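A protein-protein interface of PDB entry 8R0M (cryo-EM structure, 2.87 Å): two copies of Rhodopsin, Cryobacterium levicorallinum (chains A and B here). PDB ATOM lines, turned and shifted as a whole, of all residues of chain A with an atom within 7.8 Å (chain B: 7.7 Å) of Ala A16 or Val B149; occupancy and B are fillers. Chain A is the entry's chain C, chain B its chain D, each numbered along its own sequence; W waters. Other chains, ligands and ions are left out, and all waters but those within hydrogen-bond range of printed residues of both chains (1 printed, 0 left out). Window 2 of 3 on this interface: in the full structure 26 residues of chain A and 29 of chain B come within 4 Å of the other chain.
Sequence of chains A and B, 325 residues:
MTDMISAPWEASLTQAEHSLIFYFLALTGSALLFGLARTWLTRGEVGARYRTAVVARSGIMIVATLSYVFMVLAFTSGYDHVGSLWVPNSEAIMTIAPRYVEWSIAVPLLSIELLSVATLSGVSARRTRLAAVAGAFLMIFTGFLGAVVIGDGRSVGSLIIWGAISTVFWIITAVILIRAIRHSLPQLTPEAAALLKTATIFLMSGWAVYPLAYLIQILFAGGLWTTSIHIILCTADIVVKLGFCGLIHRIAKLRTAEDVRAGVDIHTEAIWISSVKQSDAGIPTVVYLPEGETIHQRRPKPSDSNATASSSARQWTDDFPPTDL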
ATOM      1  N   LEU A  13      34.486  37.336  22.690  1.00  0.00           N
ATOM      2  CA  LEU A  13      33.457  36.589  23.420  1.00  0.00           C
ATOM      3  C   LEU A  13      34.127  35.852  24.569  1.00  0.00           C
ATOM      4  O   LEU A  13      35.254  35.452  24.402  1.00  0.00           O
ATOM      5  CB  LEU A  13      32.858  35.647  22.374  1.00  0.00           C
ATOM      6  CG  LEU A  13      31.981  36.252  21.288  1.00  0.00           C
ATOM      7  CD1 LEU A  13      31.394  35.131  20.459  1.00  0.00           C
ATOM      8  CD2 LEU A  13      30.881  37.105  21.889  1.00  0.00           C
ATOM      9  N   THR A  14      33.446  35.695  25.695  1.00  0.00           N
ATOM     10  CA  THR A  14      33.947  34.911  26.839  1.00  0.00           C
ATOM     11  C   THR A  14      33.762  33.464  26.408  1.00  0.00           C
ATOM     12  O   THR A  14      33.557  33.255  25.237  1.00  0.00           O
ATOM     13  CB  THR A  14      33.203  35.311  28.114  1.00  0.00           C
ATOM     14  OG1 THR A  14      31.804  35.183  27.901  1.00  0.00           O
ATOM     15  CG2 THR A  14      33.504  36.725  28.547  1.00  0.00           C
ATOM     16  N   GLN A  15      33.931  32.503  27.286  1.00  0.00           N
ATOM     17  CA  GLN A  15      33.674  31.103  26.899  1.00  0.00           C
ATOM     18  C   GLN A  15      32.214  30.765  27.165  1.00  0.00           C
ATOM     19  O   GLN A  15      31.735  29.814  26.563  1.00  0.00           O
ATOM     20  CB  GLN A  15      34.623  30.203  27.676  1.00  0.00           C
ATOM     21  CG  GLN A  15      36.091  30.403  27.350  1.00  0.00           C
ATOM     22  CD  GLN A  15      36.938  29.545  28.253  1.00  0.00           C
ATOM     23  OE1 GLN A  15      37.931  29.990  28.821  1.00  0.00           O
ATOM     24  NE2 GLN A  15      36.552  28.288  28.374  1.00  0.00           N
ATOM     25  N   ALA A  16      31.536  31.490  28.044  1.00  0.00           N
ATOM     26  CA  ALA A  16      30.092  31.302  28.241  1.00  0.00           C
ATOM     27  C   ALA A  16      29.374  31.841  27.029  1.00  0.00           C
ATOM     28  O   ALA A  16      28.425  31.221  26.613  1.00  0.00           O
ATOM     29  CB  ALA A  16      29.684  32.070  29.428  1.00  0.00           C
ATOM     30  N   GLU A  17      29.829  32.973  26.504  1.00  0.00           N
ATOM     31  CA  GLU A  17      29.240  33.581  25.334  1.00  0.00           C
ATOM     32  C   GLU A  17      29.537  32.732  24.119  1.00  0.00           C
ATOM     33  O   GLU A  17      28.642  32.486  23.336  1.00  0.00           O
ATOM     34  CB  GLU A  17      29.701  35.015  25.203  1.00  0.00           C
ATOM     35  CG  GLU A  17      29.124  35.919  26.282  1.00  0.00           C
ATOM     36  CD  GLU A  17      29.889  37.242  26.451  1.00  0.00           C
ATOM     37  OE1 GLU A  17      29.518  38.067  27.334  1.00  0.00           O
ATOM     38  OE2 GLU A  17      30.907  37.454  25.721  1.00  0.00           O
ATOM     39  N   HIS A  18      30.747  32.230  24.002  1.00  0.00           N
ATOM     40  CA  HIS A  18      31.125  31.429  22.855  1.00  0.00           C
ATOM     41  C   HIS A  18      30.323  30.128  22.859  1.00  0.00           C
ATOM     42  O   HIS A  18      29.974  29.584  21.805  1.00  0.00           O
ATOM     43  CB  HIS A  18      32.638  31.221  22.885  1.00  0.00           C
ATOM     44  CG  HIS A  18      33.244  30.508  21.736  1.00  0.00           C
ATOM     45  ND1 HIS A  18      33.538  29.160  21.759  1.00  0.00           N
ATOM     46  CD2 HIS A  18      33.618  30.968  20.529  1.00  0.00           C
ATOM     47  CE1 HIS A  18      34.045  28.827  20.568  1.00  0.00           C
ATOM     48  NE2 HIS A  18      34.110  29.909  19.800  1.00  0.00           N
ATOM     49  N   SER A  19      30.064  29.557  24.021  1.00  0.00           N
ATOM     50  CA  SER A  19      29.385  28.246  24.140  1.00  0.00           C
ATOM     51  C   SER A  19      27.909  28.346  23.803  1.00  0.00           C
ATOM     52  O   SER A  19      27.424  27.445  23.144  1.00  0.00           O
ATOM     53  CB  SER A  19      29.562  27.751  25.523  1.00  0.00           C
ATOM     54  OG  SER A  19      30.927  27.541  25.822  1.00  0.00           O
ATOM     55  N   LEU A  20      27.218  29.379  24.258  1.00  0.00           N
ATOM     56  CA  LEU A  20      25.808  29.641  23.929  1.00  0.00           C
ATOM     57  C   LEU A  20      25.634  29.970  22.446  1.00  0.00           C
ATOM     58  O   LEU A  20      24.668  29.544  21.902  1.00  0.00           O
ATOM     59  CB  LEU A  20      25.396  30.793  24.829  1.00  0.00           C
ATOM     60  CG  LEU A  20      24.915  30.453  26.229  1.00  0.00           C
ATOM     61  CD1 LEU A  20      24.778  31.731  27.027  1.00  0.00           C
ATOM     62  CD2 LEU A  20      23.586  29.730  26.166  1.00  0.00           C
ATOM     63  N   ILE A  21      26.524  30.689  21.801  1.00  0.00           N
ATOM     64  CA  ILE A  21      26.449  31.014  20.345  1.00  0.00           C
ATOM     65  C   ILE A  21      26.610  29.767  19.481  1.00  0.00           C
ATOM     66  O   ILE A  21      25.976  29.742  18.463  1.00  0.00           O
ATOM     67  CB  ILE A  21      27.418  32.144  19.948  1.00  0.00           C
ATOM     68  CG1 ILE A  21      27.211  33.411  20.777  1.00  0.00           C
ATOM     69  CG2 ILE A  21      27.327  32.441  18.464  1.00  0.00           C
ATOM     70  CD1 ILE A  21      28.125  34.539  20.392  1.00  0.00           C
ATOM     71  N   PHE A  22      27.467  28.817  19.800  1.00  0.00           N
ATOM     72  CA  PHE A  22      27.539  27.538  19.063  1.00  0.00           C
ATOM     73  C   PHE A  22      26.293  26.714  19.363  1.00  0.00           C
ATOM     74  O   PHE A  22      25.800  26.081  18.453  1.00  0.00           O
ATOM     75  CB  PHE A  22      28.781  26.747  19.459  1.00  0.00           C
ATOM     76  CG  PHE A  22      28.737  25.276  19.116  1.00  0.00           C
ATOM     77  CD1 PHE A  22      29.119  24.824  17.865  1.00  0.00           C
ATOM     78  CD2 PHE A  22      28.295  24.338  20.039  1.00  0.00           C
ATOM     79  CE1 PHE A  22      29.067  23.474  17.553  1.00  0.00           C
ATOM     80  CE2 PHE A  22      28.239  22.991  19.722  1.00  0.00           C
ATOM     81  CZ  PHE A  22      28.626  22.561  18.480  1.00  0.00           C
ATOM     82  N   TYR A  23      25.798  26.695  20.587  1.00  0.00           N
ATOM     83  CA  TYR A  23      24.598  25.882  20.822  1.00  0.00           C
ATOM     84  C   TYR A  23      23.472  26.375  19.980  1.00  0.00           C
ATOM     85  O   TYR A  23      22.842  25.559  19.327  1.00  0.00           O
ATOM     86  CB  TYR A  23      24.179  26.174  22.252  1.00  0.00           C
ATOM     87  CG  TYR A  23      22.979  25.379  22.733  1.00  0.00           C
ATOM     88  CD1 TYR A  23      23.037  23.999  22.855  1.00  0.00           C
ATOM     89  CD2 TYR A  23      21.791  26.010  23.056  1.00  0.00           C
ATOM     90  CE1 TYR A  23      21.952  23.272  23.295  1.00  0.00           C
ATOM     91  CE2 TYR A  23      20.693  25.292  23.484  1.00  0.00           C
ATOM     92  CZ  TYR A  23      20.782  23.922  23.615  1.00  0.00           C
ATOM     93  OH  TYR A  23      19.716  23.202  24.046  1.00  0.00           O
ATOM     94  N   SER A  84      41.159  33.928  28.359  1.00  0.00           N
ATOM     95  CA  SER A  84      39.824  33.485  28.780  1.00  0.00           C
ATOM     96  C   SER A  84      38.806  34.077  27.799  1.00  0.00           C
ATOM     97  O   SER A  84      37.606  34.086  28.129  1.00  0.00           O
ATOM     98  CB  SER A  84      39.635  33.985  30.163  1.00  0.00           C
ATOM     99  OG  SER A  84      40.068  35.330  30.270  1.00  0.00           O
ATOM    100  N   TRP A  86      37.526  34.547  23.538  1.00  0.00           N
ATOM    101  CA  TRP A  86      37.616  34.218  22.136  1.00  0.00           C
ATOM    102  C   TRP A  86      37.662  35.515  21.346  1.00  0.00           C
ATOM    103  O   TRP A  86      36.775  36.347  21.472  1.00  0.00           O
ATOM    104  CB  TRP A  86      36.465  33.322  21.691  1.00  0.00           C
ATOM    105  CG  TRP A  86      36.439  32.022  22.419  1.00  0.00           C
ATOM    106  CD1 TRP A  86      36.055  31.797  23.703  1.00  0.00           C
ATOM    107  CD2 TRP A  86      36.898  30.768  21.898  1.00  0.00           C
ATOM    108  NE1 TRP A  86      36.198  30.472  24.006  1.00  0.00           N
ATOM    109  CE2 TRP A  86      36.720  29.829  22.924  1.00  0.00           C
ATOM    110  CE3 TRP A  86      37.433  30.363  20.678  1.00  0.00           C
ATOM    111  CZ2 TRP A  86      37.054  28.502  22.766  1.00  0.00           C
ATOM    112  CZ3 TRP A  86      37.753  29.031  20.517  1.00  0.00           C
ATOM    113  CH2 TRP A  86      37.555  28.120  21.546  1.00  0.00           C
ATOM    114  N   GLY A 223      30.119  41.650  23.839  1.00  0.00           N
ATOM    115  CA  GLY A 223      29.918  40.229  23.633  1.00  0.00           C
ATOM    116  C   GLY A 223      28.614  39.738  24.269  1.00  0.00           C
ATOM    117  O   GLY A 223      28.061  38.728  23.832  1.00  0.00           O
ATOM    118  N   THR A 227      25.869  38.113  21.763  1.00  0.00           N
ATOM    119  CA  THR A 227      25.232  36.865  22.128  1.00  0.00           C
ATOM    120  C   THR A 227      23.715  37.062  22.047  1.00  0.00           C
ATOM    121  O   THR A 227      22.979  36.242  21.506  1.00  0.00           O
ATOM    122  CB  THR A 227      25.787  36.402  23.480  1.00  0.00           C
ATOM    123  OG1 THR A 227      27.183  36.219  23.254  1.00  0.00           O
ATOM    124  CG2 THR A 227      25.204  35.100  23.982  1.00  0.00           C
ATOM    125  N   ILE A 231      21.055  34.927  19.799  1.00  0.00           N
ATOM    126  CA  ILE A 231      20.060  34.123  20.473  1.00  0.00           C
ATOM    127  C   ILE A 231      18.716  34.517  19.907  1.00  0.00           C
ATOM    128  O   ILE A 231      17.979  33.659  19.442  1.00  0.00           O
ATOM    129  CB  ILE A 231      20.106  34.262  22.006  1.00  0.00           C
ATOM    130  CG1 ILE A 231      21.318  33.513  22.581  1.00  0.00           C
ATOM    131  CG2 ILE A 231      18.813  33.759  22.622  1.00  0.00           C
ATOM    132  CD1 ILE A 231      21.530  33.735  24.068  1.00  0.00           C
ATOM    133  N   TRP B   9      36.827  17.634  29.086  1.00  0.00           N
ATOM    134  CA  TRP B   9      37.615  17.882  27.884  1.00  0.00           C
ATOM    135  C   TRP B   9      38.946  18.547  28.281  1.00  0.00           C
ATOM    136  O   TRP B   9      39.631  19.162  27.472  1.00  0.00           O
ATOM    137  CB  TRP B   9      36.786  18.750  26.914  1.00  0.00           C
ATOM    138  CG  TRP B   9      36.322  20.025  27.579  1.00  0.00           C
ATOM    139  CD1 TRP B   9      37.051  21.161  27.788  1.00  0.00           C
ATOM    140  CD2 TRP B   9      35.071  20.254  28.256  1.00  0.00           C
ATOM    141  NE1 TRP B   9      36.333  22.097  28.482  1.00  0.00           N
ATOM    142  CE2 TRP B   9      35.121  21.558  28.791  1.00  0.00           C
ATOM    143  CE3 TRP B   9      33.909  19.493  28.432  1.00  0.00           C
ATOM    144  CZ2 TRP B   9      34.053  22.110  29.482  1.00  0.00           C
ATOM    145  CZ3 TRP B   9      32.857  20.044  29.125  1.00  0.00           C
ATOM    146  CH2 TRP B   9      32.927  21.339  29.638  1.00  0.00           C
ATOM    147  N   ILE B  93      36.534  20.668  23.607  1.00  0.00           N
ATOM    148  CA  ILE B  93      35.207  20.822  24.169  1.00  0.00           C
ATOM    149  C   ILE B  93      34.167  20.469  23.112  1.00  0.00           C
ATOM    150  O   ILE B  93      33.020  20.168  23.444  1.00  0.00           O
ATOM    151  CB  ILE B  93      34.939  22.244  24.688  1.00  0.00           C
ATOM    152  CG1 ILE B  93      33.645  22.325  25.493  1.00  0.00           C
ATOM    153  CG2 ILE B  93      34.912  23.218  23.525  1.00  0.00           C
ATOM    154  CD1 ILE B  93      33.454  23.607  26.173  1.00  0.00           C
ATOM    155  N   PHE B 141      18.476  21.900  28.206  1.00  0.00           N
ATOM    156  CA  PHE B 141      19.112  23.203  28.205  1.00  0.00           C
ATOM    157  C   PHE B 141      19.640  23.518  29.605  1.00  0.00           C
ATOM    158  O   PHE B 141      20.766  23.997  29.727  1.00  0.00           O
ATOM    159  CB  PHE B 141      18.152  24.252  27.641  1.00  0.00           C
ATOM    160  CG  PHE B 141      18.751  25.623  27.516  1.00  0.00           C
ATOM    161  CD1 PHE B 141      19.649  25.897  26.497  1.00  0.00           C
ATOM    162  CD2 PHE B 141      18.471  26.613  28.452  1.00  0.00           C
ATOM    163  CE1 PHE B 141      20.258  27.143  26.412  1.00  0.00           C
ATOM    164  CE2 PHE B 141      19.082  27.851  28.368  1.00  0.00           C
ATOM    165  CZ  PHE B 141      19.977  28.111  27.356  1.00  0.00           C
ATOM    166  N   GLY B 143      20.697  21.437  31.708  1.00  0.00           N
ATOM    167  CA  GLY B 143      21.894  20.635  31.838  1.00  0.00           C
ATOM    168  C   GLY B 143      23.070  21.303  31.141  1.00  0.00           C
ATOM    169  O   GLY B 143      24.077  21.587  31.790  1.00  0.00           O
ATOM    170  N   PHE B 144      22.932  21.587  29.852  1.00  0.00           N
ATOM    171  CA  PHE B 144      23.935  22.363  29.140  1.00  0.00           C
ATOM    172  C   PHE B 144      24.527  23.521  29.962  1.00  0.00           C
ATOM    173  O   PHE B 144      25.736  23.753  29.971  1.00  0.00           O
ATOM    174  CB  PHE B 144      23.316  22.979  27.897  1.00  0.00           C
ATOM    175  CG  PHE B 144      24.295  23.618  26.970  1.00  0.00           C
ATOM    176  CD1 PHE B 144      25.337  22.886  26.437  1.00  0.00           C
ATOM    177  CD2 PHE B 144      24.162  24.944  26.617  1.00  0.00           C
ATOM    178  CE1 PHE B 144      26.214  23.471  25.538  1.00  0.00           C
ATOM    179  CE2 PHE B 144      25.059  25.533  25.742  1.00  0.00           C
ATOM    180  CZ  PHE B 144      26.085  24.799  25.216  1.00  0.00           C
ATOM    181  N   LEU B 145      23.682  24.276  30.643  1.00  0.00           N
ATOM    182  CA  LEU B 145      24.178  25.431  31.343  1.00  0.00           C
ATOM    183  C   LEU B 145      25.088  25.010  32.483  1.00  0.00           C
ATOM    184  O   LEU B 145      26.051  25.723  32.736  1.00  0.00           O
ATOM    185  CB  LEU B 145      23.004  26.266  31.859  1.00  0.00           C
ATOM    186  CG  LEU B 145      22.153  26.990  30.811  1.00  0.00           C
ATOM    187  CD1 LEU B 145      21.168  27.881  31.516  1.00  0.00           C
ATOM    188  CD2 LEU B 145      22.968  27.817  29.822  1.00  0.00           C
ATOM    189  N   GLY B 146      24.728  23.932  33.202  1.00  0.00           N
ATOM    190  CA  GLY B 146      25.513  23.412  34.317  1.00  0.00           C
ATOM    191  C   GLY B 146      26.799  22.761  33.817  1.00  0.00           C
ATOM    192  O   GLY B 146      27.903  23.022  34.303  1.00  0.00           O
ATOM    193  N   ALA B 147      26.669  22.018  32.740  1.00  0.00           N
ATOM    194  CA  ALA B 147      27.765  21.206  32.302  1.00  0.00           C
ATOM    195  C   ALA B 147      28.754  21.950  31.423  1.00  0.00           C
ATOM    196  O   ALA B 147      29.853  21.439  31.212  1.00  0.00           O
ATOM    197  CB  ALA B 147      27.208  20.070  31.510  1.00  0.00           C
ATOM    198  N   VAL B 148      28.332  23.018  30.747  1.00  0.00           N
ATOM    199  CA  VAL B 148      29.185  23.570  29.714  1.00  0.00           C
ATOM    200  C   VAL B 148      29.370  25.051  29.892  1.00  0.00           C
ATOM    201  O   VAL B 148      30.478  25.510  29.637  1.00  0.00           O
ATOM    202  CB  VAL B 148      28.689  23.278  28.298  1.00  0.00           C
ATOM    203  CG1 VAL B 148      29.528  24.008  27.259  1.00  0.00           C
ATOM    204  CG2 VAL B 148      28.715  21.783  28.035  1.00  0.00           C
ATOM    205  N   VAL B 149      28.321  25.774  30.298  1.00  0.00           N
ATOM    206  CA  VAL B 149      28.311  27.215  30.101  1.00  0.00           C
ATOM    207  C   VAL B 149      28.750  27.892  31.383  1.00  0.00           C
ATOM    208  O   VAL B 149      29.734  28.620  31.366  1.00  0.00           O
ATOM    209  CB  VAL B 149      26.965  27.711  29.550  1.00  0.00           C
ATOM    210  CG1 VAL B 149      26.810  29.203  29.733  1.00  0.00           C
ATOM    211  CG2 VAL B 149      26.753  27.291  28.086  1.00  0.00           C
ATOM    212  N   ILE B 150      28.104  27.596  32.492  1.00  0.00           N
ATOM    213  CA  ILE B 150      28.324  28.388  33.686  1.00  0.00           C
ATOM    214  C   ILE B 150      29.358  27.715  34.568  1.00  0.00           C
ATOM    215  O   ILE B 150      29.070  26.663  35.132  1.00  0.00           O
ATOM    216  CB  ILE B 150      27.002  28.506  34.448  1.00  0.00           C
ATOM    217  CG1 ILE B 150      25.947  29.145  33.552  1.00  0.00           C
ATOM    218  CG2 ILE B 150      27.202  29.245  35.749  1.00  0.00           C
ATOM    219  CD1 ILE B 150      24.581  29.172  34.165  1.00  0.00           C
ATOM    220  N   GLY B 151      30.522  28.339  34.741  1.00  0.00           N
ATOM    221  CA  GLY B 151      31.612  27.683  35.448  1.00  0.00           C
ATOM    222  C   GLY B 151      32.596  27.056  34.469  1.00  0.00           C
ATOM    223  O   GLY B 151      33.726  26.775  34.847  1.00  0.00           O
ATOM    224  N   ASP B 152      32.145  26.886  33.218  1.00  0.00           N
ATOM    225  CA  ASP B 152      32.959  26.343  32.146  1.00  0.00           C
ATOM    226  C   ASP B 152      33.138  24.842  32.340  1.00  0.00           C
ATOM    227  O   ASP B 152      34.149  24.285  31.917  1.00  0.00           O
ATOM    228  CB  ASP B 152      34.325  27.042  32.037  1.00  0.00           C
ATOM    229  CG  ASP B 152      34.256  28.525  31.704  1.00  0.00           C
ATOM    230  OD1 ASP B 152      33.167  28.986  31.261  1.00  0.00           O
ATOM    231  OD2 ASP B 152      35.291  29.213  31.894  1.00  0.00           O
ATOM    232  N   GLY B 153      32.167  24.204  33.000  1.00  0.00           N
ATOM    233  CA  GLY B 153      32.222  22.781  33.267  1.00  0.00           C
ATOM    234  C   GLY B 153      33.086  22.452  34.478  1.00  0.00           C
ATOM    235  O   GLY B 153      33.222  21.278  34.809  1.00  0.00           O
ATOM    236  N   ARG B 154      33.615  23.467  35.155  1.00  0.00           N
ATOM    237  CA  ARG B 154      34.652  23.251  36.129  1.00  0.00           C
ATOM    238  C   ARG B 154      34.133  23.651  37.488  1.00  0.00           C
ATOM    239  O   ARG B 154      34.936  23.883  38.382  1.00  0.00           O
ATOM    240  CB  ARG B 154      35.871  24.128  35.852  1.00  0.00           C
ATOM    241  CG  ARG B 154      36.597  23.861  34.547  1.00  0.00           C
ATOM    242  CD  ARG B 154      37.888  24.710  34.527  1.00  0.00           C
ATOM    243  NE  ARG B 154      38.806  24.583  35.672  1.00  0.00           N
ATOM    244  N   SER B 158      27.851  24.797  40.281  1.00  0.00           N
ATOM    245  CA  SER B 158      27.059  25.071  39.103  1.00  0.00           C
ATOM    246  C   SER B 158      26.554  23.767  38.479  1.00  0.00           C
ATOM    247  O   SER B 158      25.558  23.770  37.777  1.00  0.00           O
ATOM    248  CB  SER B 158      27.856  25.917  38.135  1.00  0.00           C
ATOM    249  OG  SER B 158      27.197  26.087  36.881  1.00  0.00           O
HETATM  250  O   HOH W   1      31.780  27.153  28.430  1.00  0.00           O
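The backbone carbonyl oxygen (O) of Gln A15 is in hydrogen-bond range of the side-chain hydroxyl (OG) of Ser A19 (2.5 Å). The backbone carbonyl oxygen of Phe B144 is in hydrogen-bond range of the backbone NH of Val B149, at 3.3 Å.
Gln A15 touches Asp B152 (NE2 to OD2, 3.9 Å). Ala A16 touches Val B149 (CB to O, 3.96 Å). Phe B144 touches Ser A19. Val B149 touches Ser A19. Tyr A23 touches Phe B141 (CE2 to CD1, 3.2 Å). Tyr A23 touches Phe B144 (CB to CE2, 3.7 Å).
Of the printed residues of chain B, Gln A15 touches Asp B152 (3.9 Å). Ala A16 touches just one residue of chain B: Val B149. Printed residues of chain B within 4 Å of Tyr A23: Phe B141 (3.2 Å) and Phe B144 (3.7 Å). Val B149 touches two residues of chain A. Of the printed residues of chain A, Asp B152 touches Gln A15 (3.9 Å).
Of the 16 printed residues of chain B, 4 touch a printed residue of chain A. Printed residues of chain B that touch a printed residue of chain A: Phe B141, Phe B144, Val B149 and Asp B152. Hydrophobic or aromatic side chains of chain B within 4 Å of the printed part of chain A: Phe B141, Phe B144 and Val B149. Of the 16 printed residues of chain A, 4 touch a printed residue of chain B. Along chain A the printed residues that touch a printed residue of chain B span positions 15 to 23.
No position is printed for both chains. Of the 6 pairs that touch across the chains among the printed residues, none has its exchanged pair printed and touching as well.
Water W1 lies within hydrogen-bond range of O of Val B148 (2.4 Å), OG of Ser A19 (2.8 Å) and O of Gln A15 (3.3 Å).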
